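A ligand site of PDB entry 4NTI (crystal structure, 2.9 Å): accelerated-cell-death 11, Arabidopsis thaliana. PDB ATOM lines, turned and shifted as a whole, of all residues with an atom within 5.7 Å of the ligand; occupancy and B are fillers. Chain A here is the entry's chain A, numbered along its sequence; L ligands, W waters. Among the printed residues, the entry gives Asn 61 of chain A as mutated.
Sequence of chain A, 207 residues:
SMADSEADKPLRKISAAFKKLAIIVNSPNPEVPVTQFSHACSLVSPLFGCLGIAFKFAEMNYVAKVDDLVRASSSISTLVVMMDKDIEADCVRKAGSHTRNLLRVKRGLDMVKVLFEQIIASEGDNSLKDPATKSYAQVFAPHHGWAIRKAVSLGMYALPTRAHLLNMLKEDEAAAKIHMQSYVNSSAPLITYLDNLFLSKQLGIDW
The guanidinium group (NE) of Arg 104 lies within salt-bridge range of an oxygen (O5) of the ligand.
NE of Arg 100 is in salt-bridge range of O5 of the ligand (2.8 Å).
A nitrogen (N1) of the ligand lies within hydrogen-bond range of the side-chain amide oxygen (OD1) of Asn 61 (2.9 Å).
A ring nitrogen (NE2) of His 144 lies within hydrogen-bond range of an oxygen (O6) of the ligand.
O4 of the ligand is in salt-bridge range of NZ of Lys 65, 3.0 Å away.
The side-chain amide oxygen (OD1) of Asn 61 is in hydrogen-bond range of the side-chain amino group (NZ) of Lys 65, 3.0 Å away.
The side-chain hydroxyl (OH) of Tyr 136 lies within hydrogen-bond range of a ring nitrogen (ND1) of His 144 (2.7 Å).
O of Ala 132 is in hydrogen-bond range of OG of Ser 135 (3.1 Å).
OG of Ser 135 sits close to SD of Met 111.
Leu 47 touches the ligand.
CZ of Phe 48 touches C26 of the ligand (3.5 Å).
Leu 51 touches the ligand (CD2 to C1, 3.5 Å).
CE1 of Phe 55 touches C5 of the ligand (3.4 Å).
Phe 57 touches the ligand.
Ala 58 touches the ligand (CB to C8, 3.8 Å).
Tyr 62 touches the ligand (CD1 to C23, 3.7 Å).
Gly 108 touches the ligand.
Met 111 touches the ligand.
Val 112 touches the ligand.
CD2 of Leu 115 touches C1 of the ligand (3.6 Å).
CB of Ala 132 touches C2 of the ligand (3.5 Å).
Tyr 136 touches the ligand.
CZ of Phe 140 touches C21 of the ligand (3.5 Å).
CG2 of Val 152 touches C9 of the ligand, at 3.9 Å.
Met 156 touches the ligand.
Hydrophobic or aromatic side chains within 4 Å of the ligand: Leu 47, Phe 48, Leu 51, Phe 55, Phe 57, Ala 58, Tyr 62, Met 111, Val 112, Leu 115, Ala 132, Tyr 136, Phe 140, His 144, Val 152 and Met 156.
21 residues have an atom within 4 Å of the ligand: Leu 47, Phe 48, Leu 51, Phe 55, Phe 57, Ala 58, Asn 61, Tyr 62, Lys 65, Arg 100, Arg 104, Gly 108, Met 111, Val 112, Leu 115, Ala 132, Tyr 136, Phe 140, His 144, Val 152 and Met 156.
The nearest printed residue that does not touch the ligand is Leu 159 (4.2 Å).
Water W2 bridges O6 of the ligand (2.7 Å) and NH1 of Arg 107 (2.8 Å).
Water W1 lies within hydrogen-bond range of OD1 of Asn 101, N of Gly 96 and O5 of the ligand.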
ATOM      1  N   VAL A  44      25.923  -2.419  -6.675  1.00  0.00           N
ATOM      2  CA  VAL A  44      24.843  -2.502  -7.655  1.00  0.00           C
ATOM      3  C   VAL A  44      24.488  -1.114  -8.180  1.00  0.00           C
ATOM      4  O   VAL A  44      24.150  -0.946  -9.355  1.00  0.00           O
ATOM      5  CB  VAL A  44      23.604  -3.204  -7.052  1.00  0.00           C
ATOM      6  CG1 VAL A  44      22.339  -2.848  -7.837  1.00  0.00           C
ATOM      7  CG2 VAL A  44      23.803  -4.701  -7.023  1.00  0.00           C
ATOM      8  N   LEU A  47      24.971   0.405 -11.639  1.00  0.00           N
ATOM      9  CA  LEU A  47      24.131  -0.059 -12.747  1.00  0.00           C
ATOM     10  C   LEU A  47      23.160   1.039 -13.174  1.00  0.00           C
ATOM     11  O   LEU A  47      22.799   1.131 -14.341  1.00  0.00           O
ATOM     12  CB  LEU A  47      23.373  -1.339 -12.392  1.00  0.00           C
ATOM     13  CG  LEU A  47      24.168  -2.639 -12.219  1.00  0.00           C
ATOM     14  CD1 LEU A  47      23.351  -3.829 -12.715  1.00  0.00           C
ATOM     15  CD2 LEU A  47      25.503  -2.574 -12.940  1.00  0.00           C
ATOM     16  N   PHE A  48      22.747   1.867 -12.218  1.00  0.00           N
ATOM     17  CA  PHE A  48      22.081   3.124 -12.544  1.00  0.00           C
ATOM     18  C   PHE A  48      23.154   4.017 -13.151  1.00  0.00           C
ATOM     19  O   PHE A  48      24.327   3.918 -12.779  1.00  0.00           O
ATOM     20  CB  PHE A  48      21.504   3.794 -11.304  1.00  0.00           C
ATOM     21  CG  PHE A  48      20.554   2.934 -10.518  1.00  0.00           C
ATOM     22  CD1 PHE A  48      19.210   2.863 -10.869  1.00  0.00           C
ATOM     23  CD2 PHE A  48      20.991   2.209  -9.429  1.00  0.00           C
ATOM     24  CE1 PHE A  48      18.332   2.073 -10.142  1.00  0.00           C
ATOM     25  CE2 PHE A  48      20.125   1.422  -8.696  1.00  0.00           C
ATOM     26  CZ  PHE A  48      18.791   1.353  -9.050  1.00  0.00           C
ATOM     27  N   LEU A  51      21.532   3.224 -17.208  1.00  0.00           N
ATOM     28  CA  LEU A  51      20.177   3.504 -17.631  1.00  0.00           C
ATOM     29  C   LEU A  51      20.110   5.007 -17.920  1.00  0.00           C
ATOM     30  O   LEU A  51      21.103   5.713 -17.731  1.00  0.00           O
ATOM     31  CB  LEU A  51      19.191   3.096 -16.535  1.00  0.00           C
ATOM     32  CG  LEU A  51      19.481   1.701 -15.955  1.00  0.00           C
ATOM     33  CD1 LEU A  51      18.394   1.249 -14.982  1.00  0.00           C
ATOM     34  CD2 LEU A  51      19.676   0.675 -17.066  1.00  0.00           C
ATOM     35  N   PHE A  55      15.557   7.082 -14.896  1.00  0.00           N
ATOM     36  CA  PHE A  55      15.560   6.218 -13.713  1.00  0.00           C
ATOM     37  C   PHE A  55      16.391   6.780 -12.570  1.00  0.00           C
ATOM     38  O   PHE A  55      16.936   6.037 -11.765  1.00  0.00           O
ATOM     39  CB  PHE A  55      16.042   4.819 -14.075  1.00  0.00           C
ATOM     40  CG  PHE A  55      15.037   4.031 -14.855  1.00  0.00           C
ATOM     41  CD1 PHE A  55      13.854   3.628 -14.263  1.00  0.00           C
ATOM     42  CD2 PHE A  55      15.258   3.723 -16.180  1.00  0.00           C
ATOM     43  CE1 PHE A  55      12.922   2.921 -14.974  1.00  0.00           C
ATOM     44  CE2 PHE A  55      14.324   3.006 -16.901  1.00  0.00           C
ATOM     45  CZ  PHE A  55      13.158   2.605 -16.294  1.00  0.00           C
ATOM     46  N   PHE A  57      15.106   8.628 -10.267  1.00  0.00           N
ATOM     47  CA  PHE A  57      14.265   8.489  -9.077  1.00  0.00           C
ATOM     48  C   PHE A  57      14.462   7.112  -8.441  1.00  0.00           C
ATOM     49  O   PHE A  57      14.417   6.973  -7.222  1.00  0.00           O
ATOM     50  CB  PHE A  57      12.784   8.766  -9.400  1.00  0.00           C
ATOM     51  CG  PHE A  57      12.123   7.695 -10.231  1.00  0.00           C
ATOM     52  CD1 PHE A  57      12.272   7.662 -11.605  1.00  0.00           C
ATOM     53  CD2 PHE A  57      11.342   6.719  -9.623  1.00  0.00           C
ATOM     54  CE1 PHE A  57      11.660   6.687 -12.357  1.00  0.00           C
ATOM     55  CE2 PHE A  57      10.730   5.745 -10.376  1.00  0.00           C
ATOM     56  CZ  PHE A  57      10.890   5.724 -11.743  1.00  0.00           C
ATOM     57  N   ALA A  58      14.667   6.099  -9.279  1.00  0.00           N
ATOM     58  CA  ALA A  58      14.955   4.752  -8.793  1.00  0.00           C
ATOM     59  C   ALA A  58      16.348   4.691  -8.183  1.00  0.00           C
ATOM     60  O   ALA A  58      16.548   4.044  -7.157  1.00  0.00           O
ATOM     61  CB  ALA A  58      14.824   3.741  -9.923  1.00  0.00           C
ATOM     62  N   ASN A  61      16.500   6.442  -4.637  1.00  0.00           N
ATOM     63  CA  ASN A  61      15.792   5.649  -3.652  1.00  0.00           C
ATOM     64  C   ASN A  61      16.618   4.446  -3.182  1.00  0.00           C
ATOM     65  O   ASN A  61      16.705   4.183  -1.979  1.00  0.00           O
ATOM     66  CB  ASN A  61      14.455   5.175  -4.217  1.00  0.00           C
ATOM     67  CG  ASN A  61      13.443   4.854  -3.134  1.00  0.00           C
ATOM     68  OD1 ASN A  61      13.283   3.706  -2.731  1.00  0.00           O
ATOM     69  ND2 ASN A  61      12.742   5.882  -2.659  1.00  0.00           N
ATOM     70  N   TYR A  62      17.225   3.740  -4.125  1.00  0.00           N
ATOM     71  CA  TYR A  62      18.036   2.565  -3.799  1.00  0.00           C
ATOM     72  C   TYR A  62      19.308   2.951  -3.050  1.00  0.00           C
ATOM     73  O   TYR A  62      19.639   2.342  -2.030  1.00  0.00           O
ATOM     74  CB  TYR A  62      18.386   1.788  -5.073  1.00  0.00           C
ATOM     75  CG  TYR A  62      19.275   0.583  -4.818  1.00  0.00           C
ATOM     76  CD1 TYR A  62      18.743  -0.624  -4.396  1.00  0.00           C
ATOM     77  CD2 TYR A  62      20.659   0.671  -5.003  1.00  0.00           C
ATOM     78  CE1 TYR A  62      19.558  -1.720  -4.157  1.00  0.00           C
ATOM     79  CE2 TYR A  62      21.468  -0.416  -4.772  1.00  0.00           C
ATOM     80  CZ  TYR A  62      20.919  -1.605  -4.355  1.00  0.00           C
ATOM     81  OH  TYR A  62      21.741  -2.690  -4.119  1.00  0.00           O
ATOM     82  N   LYS A  65      18.706   4.020   0.528  1.00  0.00           N
ATOM     83  CA  LYS A  65      18.449   2.869   1.382  1.00  0.00           C
ATOM     84  C   LYS A  65      19.729   2.090   1.695  1.00  0.00           C
ATOM     85  O   LYS A  65      19.884   1.552   2.790  1.00  0.00           O
ATOM     86  CB  LYS A  65      17.413   1.952   0.730  1.00  0.00           C
ATOM     87  CG  LYS A  65      16.001   2.480   0.817  1.00  0.00           C
ATOM     88  CD  LYS A  65      15.020   1.602   0.071  1.00  0.00           C
ATOM     89  CE  LYS A  65      13.593   2.007   0.398  1.00  0.00           C
ATOM     90  NZ  LYS A  65      13.390   3.481   0.254  1.00  0.00           N
ATOM     91  N   ALA A  95       8.753   3.919   8.380  1.00  0.00           N
ATOM     92  CA  ALA A  95       9.429   4.424   7.185  1.00  0.00           C
ATOM     93  C   ALA A  95      10.878   4.819   7.465  1.00  0.00           C
ATOM     94  O   ALA A  95      11.152   5.588   8.384  1.00  0.00           O
ATOM     95  CB  ALA A  95       8.664   5.587   6.587  1.00  0.00           C
ATOM     96  N   GLY A  96      11.787   4.289   6.656  1.00  0.00           N
ATOM     97  CA  GLY A  96      13.191   4.615   6.771  1.00  0.00           C
ATOM     98  C   GLY A  96      13.954   3.780   7.784  1.00  0.00           C
ATOM     99  O   GLY A  96      15.139   3.991   8.001  1.00  0.00           O
ATOM    100  N   ARG A 100      13.012  -2.218   7.276  1.00  0.00           N
ATOM    101  CA  ARG A 100      12.167  -1.882   6.136  1.00  0.00           C
ATOM    102  C   ARG A 100      13.015  -1.625   4.889  1.00  0.00           C
ATOM    103  O   ARG A 100      12.708  -2.133   3.811  1.00  0.00           O
ATOM    104  CB  ARG A 100      11.264  -0.680   6.439  1.00  0.00           C
ATOM    105  CG  ARG A 100      10.436  -0.213   5.249  1.00  0.00           C
ATOM    106  CD  ARG A 100       9.327   0.753   5.671  1.00  0.00           C
ATOM    107  NE  ARG A 100       8.665   1.354   4.516  1.00  0.00           N
ATOM    108  CZ  ARG A 100       7.615   2.174   4.587  1.00  0.00           C
ATOM    109  NH1 ARG A 100       7.092   2.471   5.766  1.00  0.00           N
ATOM    110  NH2 ARG A 100       7.084   2.666   3.480  1.00  0.00           N
ATOM    111  N   ASN A 101      14.076  -0.831   5.053  1.00  0.00           N
ATOM    112  CA  ASN A 101      15.016  -0.586   3.965  1.00  0.00           C
ATOM    113  C   ASN A 101      15.622  -1.886   3.440  1.00  0.00           C
ATOM    114  O   ASN A 101      15.808  -2.046   2.234  1.00  0.00           O
ATOM    115  CB  ASN A 101      16.141   0.353   4.424  1.00  0.00           C
ATOM    116  CG  ASN A 101      15.676   1.779   4.610  1.00  0.00           C
ATOM    117  OD1 ASN A 101      14.684   2.208   4.022  1.00  0.00           O
ATOM    118  ND2 ASN A 101      16.403   2.538   5.417  1.00  0.00           N
ATOM    119  N   ARG A 104      13.139  -3.650   1.116  1.00  0.00           N
ATOM    120  CA  ARG A 104      13.127  -3.004  -0.202  1.00  0.00           C
ATOM    121  C   ARG A 104      14.406  -3.295  -0.976  1.00  0.00           C
ATOM    122  O   ARG A 104      14.370  -3.563  -2.175  1.00  0.00           O
ATOM    123  CB  ARG A 104      12.910  -1.502  -0.065  1.00  0.00           C
ATOM    124  CG  ARG A 104      11.456  -1.077   0.049  1.00  0.00           C
ATOM    125  CD  ARG A 104      10.995  -1.002   1.493  1.00  0.00           C
ATOM    126  NE  ARG A 104       9.593  -0.595   1.588  1.00  0.00           N
ATOM    127  CZ  ARG A 104       8.598  -1.429   1.879  1.00  0.00           C
ATOM    128  NH1 ARG A 104       7.347  -0.978   1.939  1.00  0.00           N
ATOM    129  NH2 ARG A 104       8.845  -2.715   2.113  1.00  0.00           N
ATOM    130  N   ARG A 107      14.382  -6.656  -2.434  1.00  0.00           N
ATOM    131  CA  ARG A 107      13.624  -6.662  -3.680  1.00  0.00           C
ATOM    132  C   ARG A 107      14.473  -6.115  -4.821  1.00  0.00           C
ATOM    133  O   ARG A 107      14.344  -6.551  -5.965  1.00  0.00           O
ATOM    134  CB  ARG A 107      12.337  -5.836  -3.533  1.00  0.00           C
ATOM    135  CG  ARG A 107      11.267  -6.500  -2.683  1.00  0.00           C
ATOM    136  CD  ARG A 107      10.107  -5.554  -2.413  1.00  0.00           C
ATOM    137  NE  ARG A 107       9.128  -6.142  -1.501  1.00  0.00           N
ATOM    138  CZ  ARG A 107       8.223  -5.459  -0.822  1.00  0.00           C
ATOM    139  NH1 ARG A 107       8.155  -4.134  -0.930  1.00  0.00           N
ATOM    140  NH2 ARG A 107       7.378  -6.093  -0.023  1.00  0.00           N
ATOM    141  N   GLY A 108      15.338  -5.169  -4.501  1.00  0.00           N
ATOM    142  CA  GLY A 108      16.243  -4.592  -5.472  1.00  0.00           C
ATOM    143  C   GLY A 108      17.210  -5.631  -6.001  1.00  0.00           C
ATOM    144  O   GLY A 108      17.486  -5.692  -7.198  1.00  0.00           O
ATOM    145  N   MET A 111      15.408  -7.886  -8.210  1.00  0.00           N
ATOM    146  CA  MET A 111      15.139  -7.206  -9.466  1.00  0.00           C
ATOM    147  C   MET A 111      16.318  -7.361 -10.427  1.00  0.00           C
ATOM    148  O   MET A 111      16.128  -7.652 -11.613  1.00  0.00           O
ATOM    149  CB  MET A 111      14.866  -5.733  -9.234  1.00  0.00           C
ATOM    150  CG  MET A 111      14.743  -4.909 -10.501  1.00  0.00           C
ATOM    151  SD  MET A 111      13.420  -5.487 -11.571  1.00  0.00           S
ATOM    152  CE  MET A 111      13.379  -4.169 -12.774  1.00  0.00           C
ATOM    153  N   VAL A 112      17.520  -7.168  -9.908  1.00  0.00           N
ATOM    154  CA  VAL A 112      18.742  -7.326 -10.693  1.00  0.00           C
ATOM    155  C   VAL A 112      18.869  -8.771 -11.160  1.00  0.00           C
ATOM    156  O   VAL A 112      19.229  -9.032 -12.312  1.00  0.00           O
ATOM    157  CB  VAL A 112      19.982  -6.974  -9.848  1.00  0.00           C
ATOM    158  CG1 VAL A 112      21.260  -7.244 -10.643  1.00  0.00           C
ATOM    159  CG2 VAL A 112      19.929  -5.524  -9.387  1.00  0.00           C
ATOM    160  N   LEU A 115      16.362  -9.608 -13.905  1.00  0.00           N
ATOM    161  CA  LEU A 115      16.754  -8.837 -15.083  1.00  0.00           C
ATOM    162  C   LEU A 115      17.914  -9.505 -15.801  1.00  0.00           C
ATOM    163  O   LEU A 115      17.911  -9.632 -17.024  1.00  0.00           O
ATOM    164  CB  LEU A 115      17.150  -7.410 -14.690  1.00  0.00           C
ATOM    165  CG  LEU A 115      17.584  -6.518 -15.851  1.00  0.00           C
ATOM    166  CD1 LEU A 115      16.415  -6.234 -16.778  1.00  0.00           C
ATOM    167  CD2 LEU A 115      18.210  -5.236 -15.339  1.00  0.00           C
ATOM    168  N   LEU A 128      16.135  -3.744 -24.657  1.00  0.00           N
ATOM    169  CA  LEU A 128      16.068  -4.176 -23.269  1.00  0.00           C
ATOM    170  C   LEU A 128      14.634  -4.053 -22.757  1.00  0.00           C
ATOM    171  O   LEU A 128      14.372  -4.255 -21.575  1.00  0.00           O
ATOM    172  CB  LEU A 128      17.000  -3.339 -22.387  1.00  0.00           C
ATOM    173  CG  LEU A 128      18.502  -3.579 -22.518  1.00  0.00           C
ATOM    174  CD1 LEU A 128      19.242  -2.574 -21.664  1.00  0.00           C
ATOM    175  CD2 LEU A 128      18.861  -4.997 -22.123  1.00  0.00           C
ATOM    176  N   ALA A 132      13.479  -5.867 -19.148  1.00  0.00           N
ATOM    177  CA  ALA A 132      13.173  -4.879 -18.124  1.00  0.00           C
ATOM    178  C   ALA A 132      11.702  -4.910 -17.695  1.00  0.00           C
ATOM    179  O   ALA A 132      11.390  -4.847 -16.506  1.00  0.00           O
ATOM    180  CB  ALA A 132      13.560  -3.494 -18.590  1.00  0.00           C
ATOM    181  N   SER A 135      10.847  -8.307 -15.838  1.00  0.00           N
ATOM    182  CA  SER A 135      11.489  -8.401 -14.529  1.00  0.00           C
ATOM    183  C   SER A 135      10.860  -7.460 -13.494  1.00  0.00           C
ATOM    184  O   SER A 135      10.705  -7.823 -12.330  1.00  0.00           O
ATOM    185  CB  SER A 135      12.987  -8.130 -14.639  1.00  0.00           C
ATOM    186  OG  SER A 135      13.245  -6.757 -14.898  1.00  0.00           O
ATOM    187  N   TYR A 136      10.522  -6.239 -13.929  1.00  0.00           N
ATOM    188  CA  TYR A 136       9.864  -5.295 -13.033  1.00  0.00           C
ATOM    189  C   TYR A 136       8.492  -5.815 -12.648  1.00  0.00           C
ATOM    190  O   TYR A 136       8.046  -5.642 -11.517  1.00  0.00           O
ATOM    191  CB  TYR A 136       9.733  -3.912 -13.692  1.00  0.00           C
ATOM    192  CG  TYR A 136       8.994  -2.910 -12.831  1.00  0.00           C
ATOM    193  CD1 TYR A 136       9.666  -2.153 -11.876  1.00  0.00           C
ATOM    194  CD2 TYR A 136       7.624  -2.726 -12.971  1.00  0.00           C
ATOM    195  CE1 TYR A 136       8.985  -1.236 -11.088  1.00  0.00           C
ATOM    196  CE2 TYR A 136       6.936  -1.821 -12.181  1.00  0.00           C
ATOM    197  CZ  TYR A 136       7.627  -1.079 -11.243  1.00  0.00           C
ATOM    198  OH  TYR A 136       6.957  -0.169 -10.459  1.00  0.00           O
ATOM    199  N   PHE A 140       8.725  -5.960  -8.698  1.00  0.00           N
ATOM    200  CA  PHE A 140       8.301  -4.712  -8.069  1.00  0.00           C
ATOM    201  C   PHE A 140       6.839  -4.315  -8.294  1.00  0.00           C
ATOM    202  O   PHE A 140       6.249  -3.640  -7.443  1.00  0.00           O
ATOM    203  CB  PHE A 140       9.216  -3.558  -8.492  1.00  0.00           C
ATOM    204  CG  PHE A 140      10.465  -3.449  -7.660  1.00  0.00           C
ATOM    205  CD1 PHE A 140      10.388  -3.195  -6.302  1.00  0.00           C
ATOM    206  CD2 PHE A 140      11.718  -3.596  -8.233  1.00  0.00           C
ATOM    207  CE1 PHE A 140      11.531  -3.094  -5.527  1.00  0.00           C
ATOM    208  CE2 PHE A 140      12.864  -3.484  -7.470  1.00  0.00           C
ATOM    209  CZ  PHE A 140      12.777  -3.241  -6.119  1.00  0.00           C
ATOM    210  N   HIS A 144       4.544  -1.805  -5.881  1.00  0.00           N
ATOM    211  CA  HIS A 144       4.497  -0.387  -6.231  1.00  0.00           C
ATOM    212  C   HIS A 144       3.091   0.082  -6.583  1.00  0.00           C
ATOM    213  O   HIS A 144       2.338  -0.631  -7.253  1.00  0.00           O
ATOM    214  CB  HIS A 144       5.451  -0.092  -7.399  1.00  0.00           C
ATOM    215  CG  HIS A 144       6.910  -0.164  -7.004  1.00  0.00           C
ATOM    216  ND1 HIS A 144       7.916  -0.263  -7.956  1.00  0.00           N
ATOM    217  CD2 HIS A 144       7.508  -0.125  -5.818  1.00  0.00           C
ATOM    218  CE1 HIS A 144       9.069  -0.303  -7.333  1.00  0.00           C
ATOM    219  NE2 HIS A 144       8.867  -0.214  -6.036  1.00  0.00           N
ATOM    220  N   ILE A 148       3.681   5.047  -9.497  1.00  0.00           N
ATOM    221  CA  ILE A 148       5.043   4.539  -9.588  1.00  0.00           C
ATOM    222  C   ILE A 148       5.179   3.577 -10.762  1.00  0.00           C
ATOM    223  O   ILE A 148       6.121   3.647 -11.542  1.00  0.00           O
ATOM    224  CB  ILE A 148       5.457   3.825  -8.288  1.00  0.00           C
ATOM    225  CG1 ILE A 148       5.527   4.820  -7.125  1.00  0.00           C
ATOM    226  CG2 ILE A 148       6.800   3.125  -8.466  1.00  0.00           C
ATOM    227  CD1 ILE A 148       6.613   5.867  -7.269  1.00  0.00           C
ATOM    228  N   VAL A 152       7.317   4.205 -14.236  1.00  0.00           N
ATOM    229  CA  VAL A 152       8.308   3.210 -14.614  1.00  0.00           C
ATOM    230  C   VAL A 152       8.136   2.757 -16.062  1.00  0.00           C
ATOM    231  O   VAL A 152       9.114   2.678 -16.811  1.00  0.00           O
ATOM    232  CB  VAL A 152       8.263   1.996 -13.668  1.00  0.00           C
ATOM    233  CG1 VAL A 152       8.905   0.773 -14.312  1.00  0.00           C
ATOM    234  CG2 VAL A 152       8.942   2.328 -12.341  1.00  0.00           C
ATOM    235  N   MET A 156      10.777   3.149 -19.356  1.00  0.00           N
ATOM    236  CA  MET A 156      11.214   2.008 -20.150  1.00  0.00           C
ATOM    237  C   MET A 156      11.555   2.428 -21.574  1.00  0.00           C
ATOM    238  O   MET A 156      12.355   1.784 -22.246  1.00  0.00           O
ATOM    239  CB  MET A 156      10.128   0.932 -20.176  1.00  0.00           C
ATOM    240  CG  MET A 156       9.881   0.261 -18.838  1.00  0.00           C
ATOM    241  SD  MET A 156      11.271  -0.766 -18.319  1.00  0.00           S
ATOM    242  CE  MET A 156      10.704  -1.348 -16.727  1.00  0.00           C
ATOM    243  N   LEU A 159      15.201   3.739 -21.938  1.00  0.00           N
ATOM    244  CA  LEU A 159      16.256   2.758 -21.744  1.00  0.00           C
ATOM    245  C   LEU A 159      17.261   2.784 -22.887  1.00  0.00           C
ATOM    246  O   LEU A 159      16.913   3.152 -24.018  1.00  0.00           O
ATOM    247  CB  LEU A 159      15.655   1.354 -21.637  1.00  0.00           C
ATOM    248  CG  LEU A 159      15.091   0.943 -20.281  1.00  0.00           C
ATOM    249  CD1 LEU A 159      14.581  -0.491 -20.335  1.00  0.00           C
ATOM    250  CD2 LEU A 159      16.140   1.094 -19.195  1.00  0.00           C
ATOM    251  N   LEU A 165      24.162  -0.913 -23.185  1.00  0.00           N
ATOM    252  CA  LEU A 165      24.227  -1.249 -21.760  1.00  0.00           C
ATOM    253  C   LEU A 165      25.518  -1.994 -21.451  1.00  0.00           C
ATOM    254  O   LEU A 165      26.239  -1.656 -20.513  1.00  0.00           O
ATOM    255  CB  LEU A 165      23.039  -2.102 -21.324  1.00  0.00           C
ATOM    256  CG  LEU A 165      23.113  -2.571 -19.870  1.00  0.00           C
ATOM    257  CD1 LEU A 165      23.079  -1.377 -18.926  1.00  0.00           C
ATOM    258  CD2 LEU A 165      22.020  -3.562 -19.532  1.00  0.00           C
HETATM  259  C1  LIG L   1      17.436  -1.990 -16.708  1.00  0.00           C
HETATM  260  C2  LIG L   1      15.949  -2.139 -16.400  1.00  0.00           C
HETATM  261  C3  LIG L   1      15.515  -1.152 -15.309  1.00  0.00           C
HETATM  262  C4  LIG L   1      14.030  -1.405 -14.969  1.00  0.00           C
HETATM  263  C5  LIG L   1      13.530  -0.287 -14.035  1.00  0.00           C
HETATM  264  C6  LIG L   1      14.141  -0.454 -12.650  1.00  0.00           C
HETATM  265  C7  LIG L   1      13.002  -0.654 -11.628  1.00  0.00           C
HETATM  266  C8  LIG L   1      13.209   0.295 -10.419  1.00  0.00           C
HETATM  267  C9  LIG L   1      11.923   1.115 -10.187  1.00  0.00           C
HETATM  268  C10 LIG L   1      11.770   1.424  -8.674  1.00  0.00           C
HETATM  269  C11 LIG L   1      11.168   2.841  -8.482  1.00  0.00           C
HETATM  270  C12 LIG L   1      11.678   3.443  -7.116  1.00  0.00           C
HETATM  271  C13 LIG L   1      10.641   4.390  -6.507  1.00  0.00           C
HETATM  272  C14 LIG L   1       9.883   3.680  -5.398  1.00  0.00           C
HETATM  273  C15 LIG L   1      10.054   4.091  -4.068  1.00  0.00           C
HETATM  274  C16 LIG L   1       9.186   3.539  -2.919  1.00  0.00           C
HETATM  275  O1  LIG L   1       7.851   3.533  -3.295  1.00  0.00           O
HETATM  276  C17 LIG L   1       9.591   2.131  -2.540  1.00  0.00           C
HETATM  277  C18 LIG L   1       9.356   1.954  -1.060  1.00  0.00           C
HETATM  278  O2  LIG L   1      10.121   2.934  -0.363  1.00  0.00           O
HETATM  279  P1  LIG L   1       9.754   3.292   1.132  1.00  0.00           P
HETATM  280  O3  LIG L   1       8.449   3.985   1.083  1.00  0.00           O
HETATM  281  O4  LIG L   1      10.802   4.390   1.576  1.00  0.00           O
HETATM  282  O5  LIG L   1       9.742   2.100   2.003  1.00  0.00           O
HETATM  283  N1  LIG L   1      10.985   1.912  -2.835  1.00  0.00           N
HETATM  284  C19 LIG L   1      11.399   0.706  -3.375  1.00  0.00           C
HETATM  285  O6  LIG L   1      10.562  -0.320  -3.641  1.00  0.00           O
HETATM  286  C20 LIG L   1      12.928   0.605  -3.644  1.00  0.00           C
HETATM  287  C21 LIG L   1      13.202   0.049  -5.072  1.00  0.00           C
HETATM  288  C22 LIG L   1      14.549   0.590  -5.544  1.00  0.00           C
HETATM  289  C23 LIG L   1      15.441  -0.581  -6.035  1.00  0.00           C
HETATM  290  C24 LIG L   1      15.617  -0.463  -7.568  1.00  0.00           C
HETATM  291  C25 LIG L   1      16.526  -1.620  -8.065  1.00  0.00           C
HETATM  292  C26 LIG L   1      16.827  -1.437  -9.570  1.00  0.00           C
HETATM  293  C27 LIG L   1      17.500  -2.734 -10.087  1.00  0.00           C
HETATM  294  C28 LIG L   1      18.783  -2.411 -10.843  1.00  0.00           C
HETATM  295  C29 LIG L   1      18.555  -1.223 -11.776  1.00  0.00           C
HETATM  296  C30 LIG L   1      19.895  -0.620 -12.138  1.00  0.00           C
HETATM  297  O   HOH W   1      11.961   2.582   4.151  1.00  0.00           O
HETATM  298  O   HOH W   2       8.709  -2.070  -2.800  1.00  0.00           O
